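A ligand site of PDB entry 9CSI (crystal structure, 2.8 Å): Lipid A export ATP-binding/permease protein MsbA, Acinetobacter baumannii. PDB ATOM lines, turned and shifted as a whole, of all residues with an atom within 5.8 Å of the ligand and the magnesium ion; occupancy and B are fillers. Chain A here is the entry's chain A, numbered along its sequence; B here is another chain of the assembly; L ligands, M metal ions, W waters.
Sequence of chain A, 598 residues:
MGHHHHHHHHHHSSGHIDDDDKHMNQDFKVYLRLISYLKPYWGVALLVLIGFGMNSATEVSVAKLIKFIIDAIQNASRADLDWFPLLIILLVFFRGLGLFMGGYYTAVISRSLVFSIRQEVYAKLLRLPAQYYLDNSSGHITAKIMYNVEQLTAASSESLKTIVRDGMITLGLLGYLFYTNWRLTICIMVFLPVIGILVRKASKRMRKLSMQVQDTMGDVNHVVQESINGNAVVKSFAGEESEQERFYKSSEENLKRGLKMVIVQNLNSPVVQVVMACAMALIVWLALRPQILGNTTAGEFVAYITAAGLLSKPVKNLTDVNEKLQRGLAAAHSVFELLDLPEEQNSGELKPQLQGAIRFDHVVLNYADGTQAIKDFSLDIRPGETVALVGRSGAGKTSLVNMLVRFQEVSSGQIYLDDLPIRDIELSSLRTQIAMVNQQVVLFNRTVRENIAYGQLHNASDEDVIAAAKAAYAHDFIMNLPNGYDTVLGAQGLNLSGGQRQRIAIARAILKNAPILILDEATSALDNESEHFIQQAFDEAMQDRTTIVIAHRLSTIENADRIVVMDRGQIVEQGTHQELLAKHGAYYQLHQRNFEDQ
The side-chain hydroxyl of Ser 393 is in hydrogen-bond range of an oxygen (O1) of the ligand, at 2.6 Å. The side-chain hydroxyl (OH) of Tyr 367 sits close to a nitrogen (N3) of the ligand. O12 of the ligand lies close to O of Asn 495 of chain B (3.3 Å). A nitrogen (N6) of the ligand sits at hydrogen-bond distance from the side-chain hydroxyl (OG1) of Thr 371, at 3.1 Å. The backbone NH (N) of Thr 398 lies close to an oxygen (O5) of the ligand. NZ of Lys 397 lies within salt-bridge range of O4 of the ligand, 2.8 Å away. N of Gly 498 of chain B lies within hydrogen-bond range of O1 of the ligand (3.0 Å). An oxygen (O4) of the ligand lies within hydrogen-bond range of the backbone NH of Lys 397 (2.8 Å). An oxygen (O7) of the ligand lies within hydrogen-bond range of the backbone NH (N) of Ser 399 (2.8 Å). N of Gly 396 lies within hydrogen-bond range of O4 of the ligand (3.1 Å). The backbone NH (N) of Gly 499 of chain B lies within hydrogen-bond range of an oxygen (O1) of the ligand. The side-chain hydroxyl (OG) of Ser 497 of chain B sits at hydrogen-bond distance from an oxygen (O1) of the ligand (3.1 Å). An oxygen (O7) of the ligand lies within hydrogen-bond range of the side-chain hydroxyl (OG) of Ser 399 (2.7 Å). O12 of the ligand is in hydrogen-bond range of OE1 of Gln 500 of chain B (2.7 Å).
N of Thr 371 sits at hydrogen-bond distance from OD1 of Asp 369. N of Ser 497 of chain B is in hydrogen-bond range of OE1 of Gln 500 of chain B (2.9 Å). The side-chain amide nitrogen of Gln 408 lies within hydrogen-bond range of the side-chain amide oxygen of Gln 131 (3.5 Å). The backbone NH (N) of Gly 499 of chain B lies close to the backbone carbonyl oxygen (O) of Ala 525 of chain B. The side-chain carboxylate of Asp 520 sits close to the side-chain hydroxyl of Thr 398 (2.7 Å). The side-chain amino group (NZ) of Lys 397 is in hydrogen-bond range of the backbone carbonyl oxygen (O) of Arg 392 (2.8 Å). The side-chain hydroxyl (OG) of Ser 399 lies within hydrogen-bond range of the side-chain hydroxyl (OH) of Tyr 367. N of Gln 439 lies close to O of Asp 520 (3.3 Å).
The backbone NH (N) of Gly 394 lies close to a nitrogen (N1) of the ligand, 3.3 Å away. Residues that only touch the ligand: Asp 369 (3.1 Å), Leu 134 (3.3 Å), Ala 395 (3.5 Å), Leu 496 of chain B (3.6 Å), Gln 131 (3.6 Å), Ala 373 (3.8 Å) and Arg 392 (3.9 Å). Hydrophobic or aromatic side chains that line the ligand: Leu 134, Tyr 367, Ala 373 and Ala 395. Within 4 Å of the ligand: Gln 131, Leu 134, Tyr 367, Asp 369, Thr 371, Ala 373, Arg 392, Ser 393, Gly 394, Ala 395, Gly 396, Lys 397, Thr 398, Ser 399, Gln 439, Asn 495 of chain B, Leu 496 of chain B, Ser 497 of chain B, Gly 498 of chain B, Gly 499 of chain B and Gln 500 of chain B.
Asp 520 touches the magnesium ion (OD1 to MG, 3.7 Å). The nearest printed residue that does not touch the magnesium ion is Gly 498 of chain B (4.4 Å).
The magnesium ion is bound by an oxygen (O3) of the ligand (1.9 Å). The magnesium ion is bound by water W4 (1.9 Å). OG1 of Thr 398 binds the magnesium ion (2.0 Å). The magnesium ion is bound by the side-chain amide nitrogen (NE2) of Gln 439 (2.2 Å). Water W6 binds the magnesium ion. O5 of the ligand binds the magnesium ion (2.3 Å). The magnesium ion has six donor atoms within binding distance.
Water W6 lies within hydrogen-bond range of O6 of the ligand (2.6 Å) and N of Gly 498 of chain B (3.1 Å). Water W5 lies within hydrogen-bond range of O2 of the ligand, OE1 of Gln 439 and OE1 of Glu 521. Water W2 lies within hydrogen-bond range of the side-chain amide nitrogen of Gln 131, a nitrogen (N5) of the ligand and the backbone NH of Asp 369.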
ATOM      1  N   GLN A 131     -14.741  29.702 -21.809  1.00  0.00           N
ATOM      2  CA  GLN A 131     -15.572  28.979 -22.763  1.00  0.00           C
ATOM      3  C   GLN A 131     -16.364  29.969 -23.634  1.00  0.00           C
ATOM      4  O   GLN A 131     -16.480  29.728 -24.835  1.00  0.00           O
ATOM      5  CB  GLN A 131     -16.481  27.931 -22.078  1.00  0.00           C
ATOM      6  CG  GLN A 131     -17.037  26.840 -23.018  1.00  0.00           C
ATOM      7  CD  GLN A 131     -15.984  25.940 -23.633  1.00  0.00           C
ATOM      8  OE1 GLN A 131     -15.239  25.220 -22.928  1.00  0.00           O
ATOM      9  NE2 GLN A 131     -15.879  25.937 -24.977  1.00  0.00           N
ATOM     10  N   LEU A 134     -14.327  31.108 -26.480  1.00  0.00           N
ATOM     11  CA  LEU A 134     -14.079  29.937 -27.322  1.00  0.00           C
ATOM     12  C   LEU A 134     -15.274  29.641 -28.252  1.00  0.00           C
ATOM     13  O   LEU A 134     -15.081  29.467 -29.449  1.00  0.00           O
ATOM     14  CB  LEU A 134     -13.797  28.728 -26.431  1.00  0.00           C
ATOM     15  CG  LEU A 134     -12.524  27.981 -26.716  1.00  0.00           C
ATOM     16  CD1 LEU A 134     -11.349  28.578 -25.945  1.00  0.00           C
ATOM     17  CD2 LEU A 134     -12.705  26.531 -26.405  1.00  0.00           C
ATOM     18  N   TYR A 367     -15.790  19.214 -20.144  1.00  0.00           N
ATOM     19  CA  TYR A 367     -15.958  20.417 -20.935  1.00  0.00           C
ATOM     20  C   TYR A 367     -17.408  20.569 -21.289  1.00  0.00           C
ATOM     21  O   TYR A 367     -18.117  19.568 -21.383  1.00  0.00           O
ATOM     22  CB  TYR A 367     -15.098  20.368 -22.190  1.00  0.00           C
ATOM     23  CG  TYR A 367     -13.653  20.711 -21.935  1.00  0.00           C
ATOM     24  CD1 TYR A 367     -13.271  22.028 -21.680  1.00  0.00           C
ATOM     25  CD2 TYR A 367     -12.673  19.718 -21.948  1.00  0.00           C
ATOM     26  CE1 TYR A 367     -11.945  22.357 -21.442  1.00  0.00           C
ATOM     27  CE2 TYR A 367     -11.330  20.045 -21.739  1.00  0.00           C
ATOM     28  CZ  TYR A 367     -10.977  21.362 -21.476  1.00  0.00           C
ATOM     29  OH  TYR A 367      -9.664  21.690 -21.249  1.00  0.00           O
ATOM     30  N   ALA A 368     -17.867  21.817 -21.461  1.00  0.00           N
ATOM     31  CA  ALA A 368     -19.247  22.165 -21.803  1.00  0.00           C
ATOM     32  C   ALA A 368     -19.869  21.096 -22.720  1.00  0.00           C
ATOM     33  O   ALA A 368     -20.935  20.549 -22.399  1.00  0.00           O
ATOM     34  CB  ALA A 368     -19.274  23.532 -22.452  1.00  0.00           C
ATOM     35  N   ASP A 369     -19.165  20.733 -23.818  1.00  0.00           N
ATOM     36  CA  ASP A 369     -19.535  19.739 -24.827  1.00  0.00           C
ATOM     37  C   ASP A 369     -19.606  18.262 -24.353  1.00  0.00           C
ATOM     38  O   ASP A 369     -19.836  17.365 -25.182  1.00  0.00           O
ATOM     39  CB  ASP A 369     -18.572  19.869 -26.035  1.00  0.00           C
ATOM     40  CG  ASP A 369     -17.148  19.349 -25.840  1.00  0.00           C
ATOM     41  OD1 ASP A 369     -16.857  18.758 -24.780  1.00  0.00           O
ATOM     42  OD2 ASP A 369     -16.346  19.508 -26.771  1.00  0.00           O
ATOM     43  N   THR A 371     -17.005  16.438 -23.132  1.00  0.00           N
ATOM     44  CA  THR A 371     -15.741  15.699 -23.175  1.00  0.00           C
ATOM     45  C   THR A 371     -15.145  15.648 -21.793  1.00  0.00           C
ATOM     46  O   THR A 371     -15.139  16.655 -21.065  1.00  0.00           O
ATOM     47  CB  THR A 371     -14.719  16.124 -24.263  1.00  0.00           C
ATOM     48  OG1 THR A 371     -14.296  17.467 -24.099  1.00  0.00           O
ATOM     49  CG2 THR A 371     -15.210  15.883 -25.673  1.00  0.00           C
ATOM     50  N   ALA A 373     -11.945  15.422 -20.224  1.00  0.00           N
ATOM     51  CA  ALA A 373     -10.490  15.654 -20.359  1.00  0.00           C
ATOM     52  C   ALA A 373      -9.640  15.104 -19.213  1.00  0.00           C
ATOM     53  O   ALA A 373      -8.515  14.677 -19.465  1.00  0.00           O
ATOM     54  CB  ALA A 373     -10.204  17.133 -20.565  1.00  0.00           C
ATOM     55  N   GLY A 391       3.139  13.063 -21.574  1.00  0.00           N
ATOM     56  CA  GLY A 391       2.132  12.195 -22.149  1.00  0.00           C
ATOM     57  C   GLY A 391       1.781  12.591 -23.564  1.00  0.00           C
ATOM     58  O   GLY A 391       2.252  13.620 -24.067  1.00  0.00           O
ATOM     59  N   ARG A 392       0.925  11.783 -24.216  1.00  0.00           N
ATOM     60  CA  ARG A 392       0.470  12.019 -25.579  1.00  0.00           C
ATOM     61  C   ARG A 392      -0.379  13.282 -25.659  1.00  0.00           C
ATOM     62  O   ARG A 392      -0.775  13.858 -24.636  1.00  0.00           O
ATOM     63  CB  ARG A 392      -0.422  10.869 -26.042  1.00  0.00           C
ATOM     64  CG  ARG A 392       0.280   9.633 -26.521  1.00  0.00           C
ATOM     65  CD  ARG A 392      -0.797   8.673 -26.969  1.00  0.00           C
ATOM     66  NE  ARG A 392      -0.314   7.296 -26.973  1.00  0.00           N
ATOM     67  CZ  ARG A 392      -0.328   6.497 -25.919  1.00  0.00           C
ATOM     68  NH1 ARG A 392      -0.791   6.924 -24.752  1.00  0.00           N
ATOM     69  NH2 ARG A 392       0.170   5.267 -26.010  1.00  0.00           N
ATOM     70  N   SER A 393      -0.707  13.678 -26.901  1.00  0.00           N
ATOM     71  CA  SER A 393      -1.598  14.808 -27.130  1.00  0.00           C
ATOM     72  C   SER A 393      -2.929  14.226 -26.743  1.00  0.00           C
ATOM     73  O   SER A 393      -3.214  13.062 -27.049  1.00  0.00           O
ATOM     74  CB  SER A 393      -1.570  15.201 -28.598  1.00  0.00           C
ATOM     75  OG  SER A 393      -2.273  16.422 -28.713  1.00  0.00           O
ATOM     76  N   GLY A 394      -3.728  14.961 -26.019  1.00  0.00           N
ATOM     77  CA  GLY A 394      -4.985  14.366 -25.574  1.00  0.00           C
ATOM     78  C   GLY A 394      -4.861  13.686 -24.213  1.00  0.00           C
ATOM     79  O   GLY A 394      -5.787  13.001 -23.774  1.00  0.00           O
ATOM     80  N   ALA A 395      -3.745  13.894 -23.521  1.00  0.00           N
ATOM     81  CA  ALA A 395      -3.540  13.371 -22.182  1.00  0.00           C
ATOM     82  C   ALA A 395      -4.315  14.236 -21.149  1.00  0.00           C
ATOM     83  O   ALA A 395      -4.757  13.729 -20.111  1.00  0.00           O
ATOM     84  CB  ALA A 395      -2.051  13.374 -21.853  1.00  0.00           C
ATOM     85  N   GLY A 396      -4.461  15.526 -21.465  1.00  0.00           N
ATOM     86  CA  GLY A 396      -5.141  16.524 -20.653  1.00  0.00           C
ATOM     87  C   GLY A 396      -4.179  17.352 -19.804  1.00  0.00           C
ATOM     88  O   GLY A 396      -4.538  17.761 -18.697  1.00  0.00           O
ATOM     89  N   LYS A 397      -2.968  17.588 -20.320  1.00  0.00           N
ATOM     90  CA  LYS A 397      -1.915  18.336 -19.626  1.00  0.00           C
ATOM     91  C   LYS A 397      -2.308  19.811 -19.527  1.00  0.00           C
ATOM     92  O   LYS A 397      -2.361  20.371 -18.426  1.00  0.00           O
ATOM     93  CB  LYS A 397      -0.557  18.109 -20.289  1.00  0.00           C
ATOM     94  CG  LYS A 397      -0.146  16.615 -20.425  1.00  0.00           C
ATOM     95  CD  LYS A 397       1.136  16.465 -21.254  1.00  0.00           C
ATOM     96  CE  LYS A 397       1.113  17.032 -22.686  1.00  0.00           C
ATOM     97  NZ  LYS A 397       0.247  16.246 -23.624  1.00  0.00           N
ATOM     98  N   THR A 398      -2.631  20.429 -20.654  1.00  0.00           N
ATOM     99  CA  THR A 398      -3.089  21.821 -20.701  1.00  0.00           C
ATOM    100  C   THR A 398      -4.378  21.977 -19.873  1.00  0.00           C
ATOM    101  O   THR A 398      -4.459  22.918 -19.082  1.00  0.00           O
ATOM    102  CB  THR A 398      -3.234  22.227 -22.143  1.00  0.00           C
ATOM    103  OG1 THR A 398      -1.930  22.124 -22.703  1.00  0.00           O
ATOM    104  CG2 THR A 398      -3.811  23.614 -22.319  1.00  0.00           C
ATOM    105  N   SER A 399      -5.342  21.022 -20.001  1.00  0.00           N
ATOM    106  CA  SER A 399      -6.622  20.960 -19.278  1.00  0.00           C
ATOM    107  C   SER A 399      -6.447  21.066 -17.733  1.00  0.00           C
ATOM    108  O   SER A 399      -7.198  21.780 -17.074  1.00  0.00           O
ATOM    109  CB  SER A 399      -7.319  19.647 -19.596  1.00  0.00           C
ATOM    110  OG  SER A 399      -7.907  19.683 -20.874  1.00  0.00           O
ATOM    111  N   LEU A 400      -5.434  20.331 -17.209  1.00  0.00           N
ATOM    112  CA  LEU A 400      -5.058  20.228 -15.797  1.00  0.00           C
ATOM    113  C   LEU A 400      -4.502  21.532 -15.276  1.00  0.00           C
ATOM    114  O   LEU A 400      -4.959  22.055 -14.260  1.00  0.00           O
ATOM    115  CB  LEU A 400      -4.039  19.100 -15.579  1.00  0.00           C
ATOM    116  CG  LEU A 400      -3.789  18.692 -14.120  1.00  0.00           C
ATOM    117  CD1 LEU A 400      -4.897  17.755 -13.593  1.00  0.00           C
ATOM    118  CD2 LEU A 400      -2.443  18.064 -13.968  1.00  0.00           C
ATOM    119  N   GLN A 408     -10.868  26.826 -16.383  1.00  0.00           N
ATOM    120  CA  GLN A 408     -11.835  25.729 -16.393  1.00  0.00           C
ATOM    121  C   GLN A 408     -12.115  25.351 -14.975  1.00  0.00           C
ATOM    122  O   GLN A 408     -11.187  25.107 -14.203  1.00  0.00           O
ATOM    123  CB  GLN A 408     -11.333  24.514 -17.182  1.00  0.00           C
ATOM    124  CG  GLN A 408     -11.448  24.669 -18.703  1.00  0.00           C
ATOM    125  CD  GLN A 408     -12.849  24.972 -19.233  1.00  0.00           C
ATOM    126  OE1 GLN A 408     -13.900  24.646 -18.614  1.00  0.00           O
ATOM    127  NE2 GLN A 408     -12.892  25.612 -20.413  1.00  0.00           N
ATOM    128  N   GLN A 439       0.565  27.530 -24.014  1.00  0.00           N
ATOM    129  CA  GLN A 439       1.062  26.742 -25.167  1.00  0.00           C
ATOM    130  C   GLN A 439       1.121  27.581 -26.494  1.00  0.00           C
ATOM    131  O   GLN A 439       2.104  27.496 -27.251  1.00  0.00           O
ATOM    132  CB  GLN A 439       0.256  25.430 -25.341  1.00  0.00           C
ATOM    133  CG  GLN A 439       0.998  24.323 -26.065  1.00  0.00           C
ATOM    134  CD  GLN A 439       0.246  23.018 -26.196  1.00  0.00           C
ATOM    135  OE1 GLN A 439       0.776  21.999 -26.673  1.00  0.00           O
ATOM    136  NE2 GLN A 439      -0.995  23.012 -25.780  1.00  0.00           N
ATOM    137  N   GLN A 440       0.072  28.392 -26.727  1.00  0.00           N
ATOM    138  CA  GLN A 440      -0.082  29.290 -27.874  1.00  0.00           C
ATOM    139  C   GLN A 440       0.138  30.680 -27.266  1.00  0.00           C
ATOM    140  O   GLN A 440      -0.730  31.164 -26.538  1.00  0.00           O
ATOM    141  CB  GLN A 440      -1.511  29.188 -28.500  1.00  0.00           C
ATOM    142  CG  GLN A 440      -1.993  27.765 -28.900  1.00  0.00           C
ATOM    143  CD  GLN A 440      -2.551  26.933 -27.751  1.00  0.00           C
ATOM    144  OE1 GLN A 440      -2.967  27.449 -26.692  1.00  0.00           O
ATOM    145  NE2 GLN A 440      -2.582  25.620 -27.941  1.00  0.00           N
ATOM    146  N   ASP A 520       3.733  25.723 -20.078  1.00  0.00           N
ATOM    147  CA  ASP A 520       3.057  24.866 -21.055  1.00  0.00           C
ATOM    148  C   ASP A 520       3.698  25.017 -22.430  1.00  0.00           C
ATOM    149  O   ASP A 520       3.396  25.951 -23.178  1.00  0.00           O
ATOM    150  CB  ASP A 520       1.546  25.133 -21.084  1.00  0.00           C
ATOM    151  CG  ASP A 520       0.734  24.100 -21.837  1.00  0.00           C
ATOM    152  OD1 ASP A 520       1.308  23.046 -22.206  1.00  0.00           O
ATOM    153  OD2 ASP A 520      -0.466  24.339 -22.053  1.00  0.00           O
ATOM    154  N   GLU A 521       4.625  24.100 -22.749  1.00  0.00           N
ATOM    155  CA  GLU A 521       5.371  24.076 -24.005  1.00  0.00           C
ATOM    156  C   GLU A 521       5.987  25.445 -24.315  1.00  0.00           C
ATOM    157  O   GLU A 521       5.828  26.006 -25.413  1.00  0.00           O
ATOM    158  CB  GLU A 521       4.516  23.530 -25.132  1.00  0.00           C
ATOM    159  CG  GLU A 521       4.252  22.039 -25.034  1.00  0.00           C
ATOM    160  CD  GLU A 521       5.454  21.115 -25.000  1.00  0.00           C
ATOM    161  OE1 GLU A 521       5.255  19.948 -24.583  1.00  0.00           O
ATOM    162  OE2 GLU A 521       6.571  21.526 -25.392  1.00  0.00           O
ATOM    163  N   ILE A 550       5.242  21.425 -18.792  1.00  0.00           N
ATOM    164  CA  ILE A 550       4.662  20.544 -19.810  1.00  0.00           C
ATOM    165  C   ILE A 550       5.671  20.650 -20.941  1.00  0.00           C
ATOM    166  O   ILE A 550       5.762  21.700 -21.584  1.00  0.00           O
ATOM    167  CB  ILE A 550       3.193  20.834 -20.253  1.00  0.00           C
ATOM    168  CG1 ILE A 550       2.207  20.779 -19.065  1.00  0.00           C
ATOM    169  CG2 ILE A 550       2.777  19.837 -21.325  1.00  0.00           C
ATOM    170  CD1 ILE A 550       0.913  21.490 -19.303  1.00  0.00           C
ATOM    171  N   LEU B 481     -14.115  13.383 -30.981  1.00  0.00           N
ATOM    172  CA  LEU B 481     -14.729  14.693 -30.676  1.00  0.00           C
ATOM    173  C   LEU B 481     -16.268  14.577 -30.621  1.00  0.00           C
ATOM    174  O   LEU B 481     -16.823  13.679 -31.261  1.00  0.00           O
ATOM    175  CB  LEU B 481     -14.316  15.776 -31.714  1.00  0.00           C
ATOM    176  CG  LEU B 481     -12.834  16.014 -32.039  1.00  0.00           C
ATOM    177  CD1 LEU B 481     -12.692  16.805 -33.304  1.00  0.00           C
ATOM    178  CD2 LEU B 481     -12.092  16.692 -30.905  1.00  0.00           C
ATOM    179  N   LEU B 494      -9.226  26.432 -30.393  1.00  0.00           N
ATOM    180  CA  LEU B 494      -8.708  26.261 -29.043  1.00  0.00           C
ATOM    181  C   LEU B 494      -9.548  25.309 -28.173  1.00  0.00           C
ATOM    182  O   LEU B 494      -9.291  25.184 -26.968  1.00  0.00           O
ATOM    183  CB  LEU B 494      -8.427  27.625 -28.377  1.00  0.00           C
ATOM    184  CG  LEU B 494      -7.208  28.385 -28.976  1.00  0.00           C
ATOM    185  CD1 LEU B 494      -7.194  29.847 -28.614  1.00  0.00           C
ATOM    186  CD2 LEU B 494      -5.889  27.710 -28.619  1.00  0.00           C
ATOM    187  N   ASN B 495     -10.492  24.585 -28.821  1.00  0.00           N
ATOM    188  CA  ASN B 495     -11.316  23.535 -28.230  1.00  0.00           C
ATOM    189  C   ASN B 495     -10.567  22.197 -28.512  1.00  0.00           C
ATOM    190  O   ASN B 495     -10.944  21.119 -28.028  1.00  0.00           O
ATOM    191  CB  ASN B 495     -12.749  23.565 -28.771  1.00  0.00           C
ATOM    192  CG  ASN B 495     -12.870  23.465 -30.272  1.00  0.00           C
ATOM    193  OD1 ASN B 495     -12.088  24.037 -31.031  1.00  0.00           O
ATOM    194  ND2 ASN B 495     -13.877  22.741 -30.723  1.00  0.00           N
ATOM    195  N   LEU B 496      -9.470  22.293 -29.273  1.00  0.00           N
ATOM    196  CA  LEU B 496      -8.565  21.178 -29.570  1.00  0.00           C
ATOM    197  C   LEU B 496      -7.249  21.446 -28.840  1.00  0.00           C
ATOM    198  O   LEU B 496      -6.904  22.593 -28.568  1.00  0.00           O
ATOM    199  CB  LEU B 496      -8.260  21.047 -31.077  1.00  0.00           C
ATOM    200  CG  LEU B 496      -9.399  20.833 -32.052  1.00  0.00           C
ATOM    201  CD1 LEU B 496      -8.870  20.759 -33.439  1.00  0.00           C
ATOM    202  CD2 LEU B 496     -10.162  19.574 -31.735  1.00  0.00           C
ATOM    203  N   SER B 497      -6.498  20.381 -28.569  1.00  0.00           N
ATOM    204  CA  SER B 497      -5.203  20.445 -27.928  1.00  0.00           C
ATOM    205  C   SER B 497      -4.161  20.966 -28.935  1.00  0.00           C
ATOM    206  O   SER B 497      -4.455  21.127 -30.126  1.00  0.00           O
ATOM    207  CB  SER B 497      -4.842  19.075 -27.386  1.00  0.00           C
ATOM    208  OG  SER B 497      -4.471  18.191 -28.415  1.00  0.00           O
ATOM    209  N   GLY B 498      -2.958  21.275 -28.431  1.00  0.00           N
ATOM    210  CA  GLY B 498      -1.848  21.825 -29.204  1.00  0.00           C
ATOM    211  C   GLY B 498      -1.495  21.045 -30.438  1.00  0.00           C
ATOM    212  O   GLY B 498      -1.617  21.584 -31.551  1.00  0.00           O
ATOM    213  N   GLY B 499      -1.065  19.784 -30.237  1.00  0.00           N
ATOM    214  CA  GLY B 499      -0.698  18.848 -31.291  1.00  0.00           C
ATOM    215  C   GLY B 499      -1.865  18.526 -32.205  1.00  0.00           C
ATOM    216  O   GLY B 499      -1.675  18.232 -33.388  1.00  0.00           O
ATOM    217  N   GLN B 500      -3.097  18.601 -31.656  1.00  0.00           N
ATOM    218  CA  GLN B 500      -4.335  18.340 -32.401  1.00  0.00           C
ATOM    219  C   GLN B 500      -4.596  19.428 -33.417  1.00  0.00           C
ATOM    220  O   GLN B 500      -4.854  19.090 -34.567  1.00  0.00           O
ATOM    221  CB  GLN B 500      -5.540  18.163 -31.467  1.00  0.00           C
ATOM    222  CG  GLN B 500      -5.632  16.783 -30.835  1.00  0.00           C
ATOM    223  CD  GLN B 500      -6.753  16.694 -29.835  1.00  0.00           C
ATOM    224  OE1 GLN B 500      -7.342  17.695 -29.431  1.00  0.00           O
ATOM    225  NE2 GLN B 500      -7.051  15.473 -29.378  1.00  0.00           N
ATOM    226  N   ALA B 525       4.490  20.743 -31.739  1.00  0.00           N
ATOM    227  CA  ALA B 525       3.488  20.461 -30.717  1.00  0.00           C
ATOM    228  C   ALA B 525       3.092  18.994 -30.672  1.00  0.00           C
ATOM    229  O   ALA B 525       2.201  18.635 -29.896  1.00  0.00           O
ATOM    230  CB  ALA B 525       2.264  21.342 -30.920  1.00  0.00           C
ATOM    231  N   ASP B 527       3.646  14.835 -30.017  1.00  0.00           N
ATOM    232  CA  ASP B 527       4.171  13.780 -29.147  1.00  0.00           C
ATOM    233  C   ASP B 527       4.995  12.809 -30.002  1.00  0.00           C
ATOM    234  O   ASP B 527       4.865  12.814 -31.224  1.00  0.00           O
ATOM    235  CB  ASP B 527       3.009  13.041 -28.446  1.00  0.00           C
ATOM    236  CG  ASP B 527       1.874  12.646 -29.379  1.00  0.00           C
ATOM    237  OD1 ASP B 527       1.181  13.547 -29.900  1.00  0.00           O
ATOM    238  OD2 ASP B 527       1.669  11.441 -29.574  1.00  0.00           O
HETATM  239  P1  LIG L   1      -1.117  18.590 -26.313  1.00  0.00           P
HETATM  240  O1  LIG L   1      -1.539  18.725 -27.692  1.00  0.00           O
HETATM  241  O2  LIG L   1       0.217  17.733 -26.287  1.00  0.00           O
HETATM  242  O3  LIG L   1      -0.890  20.055 -25.744  1.00  0.00           O
HETATM  243  P2  LIG L   1      -2.813  18.096 -23.933  1.00  0.00           P
HETATM  244  O4  LIG L   1      -2.325  17.064 -23.038  1.00  0.00           O
HETATM  245  O5  LIG L   1      -2.305  19.509 -23.499  1.00  0.00           O
HETATM  246  N1  LIG L   1      -2.276  17.842 -25.450  1.00  0.00           N
HETATM  247  P3  LIG L   1      -5.561  19.115 -23.707  1.00  0.00           P
HETATM  248  O6  LIG L   1      -5.344  20.417 -24.361  1.00  0.00           O
HETATM  249  O7  LIG L   1      -5.621  19.384 -22.229  1.00  0.00           O
HETATM  250  O8  LIG L   1      -4.372  18.092 -23.954  1.00  0.00           O
HETATM  251  O9  LIG L   1      -6.928  18.378 -24.061  1.00  0.00           O
HETATM  252  C1  LIG L   1      -7.214  16.983 -23.805  1.00  0.00           C
HETATM  253  C2  LIG L   1      -8.453  16.652 -24.601  1.00  0.00           C
HETATM  254  O10 LIG L   1      -9.495  17.609 -24.275  1.00  0.00           O
HETATM  255  C3  LIG L   1      -8.308  16.699 -26.131  1.00  0.00           C
HETATM  256  O11 LIG L   1      -8.918  15.589 -26.800  1.00  0.00           O
HETATM  257  C4  LIG L   1      -8.901  18.063 -26.498  1.00  0.00           C
HETATM  258  O12 LIG L   1      -9.420  18.210 -27.814  1.00  0.00           O
HETATM  259  C5  LIG L   1      -9.991  18.222 -25.454  1.00  0.00           C
HETATM  260  N2  LIG L   1     -10.317  19.617 -25.159  1.00  0.00           N
HETATM  261  C6  LIG L   1      -9.435  20.606 -24.789  1.00  0.00           C
HETATM  262  N3  LIG L   1      -9.976  21.782 -24.655  1.00  0.00           N
HETATM  263  C7  LIG L   1     -11.311  21.568 -24.937  1.00  0.00           C
HETATM  264  C8  LIG L   1     -12.434  22.420 -24.938  1.00  0.00           C
HETATM  265  N4  LIG L   1     -12.375  23.728 -24.624  1.00  0.00           N
HETATM  266  N5  LIG L   1     -13.635  21.886 -25.243  1.00  0.00           N
HETATM  267  C9  LIG L   1     -13.703  20.588 -25.528  1.00  0.00           C
HETATM  268  N6  LIG L   1     -12.718  19.672 -25.560  1.00  0.00           N
HETATM  269  C10 LIG L   1     -11.539  20.241 -25.250  1.00  0.00           C
HETATM  270 MG    MG M   1      -1.195  21.389 -24.360  1.00  0.00          MG
HETATM  271  O   HOH W   1     -10.251  13.749 -29.272  1.00  0.00           O
HETATM  272  O   HOH W   2     -16.797  22.862 -25.153  1.00  0.00           O
HETATM  273  O   HOH W   3      -7.101  22.337 -24.271  1.00  0.00           O
HETATM  274  O   HOH W   4       0.354  20.779 -23.348  1.00  0.00           O
HETATM  275  O   HOH W   5       2.157  19.747 -25.115  1.00  0.00           O
HETATM  276  O   HOH W   6      -3.163  21.462 -25.297  1.00  0.00           O
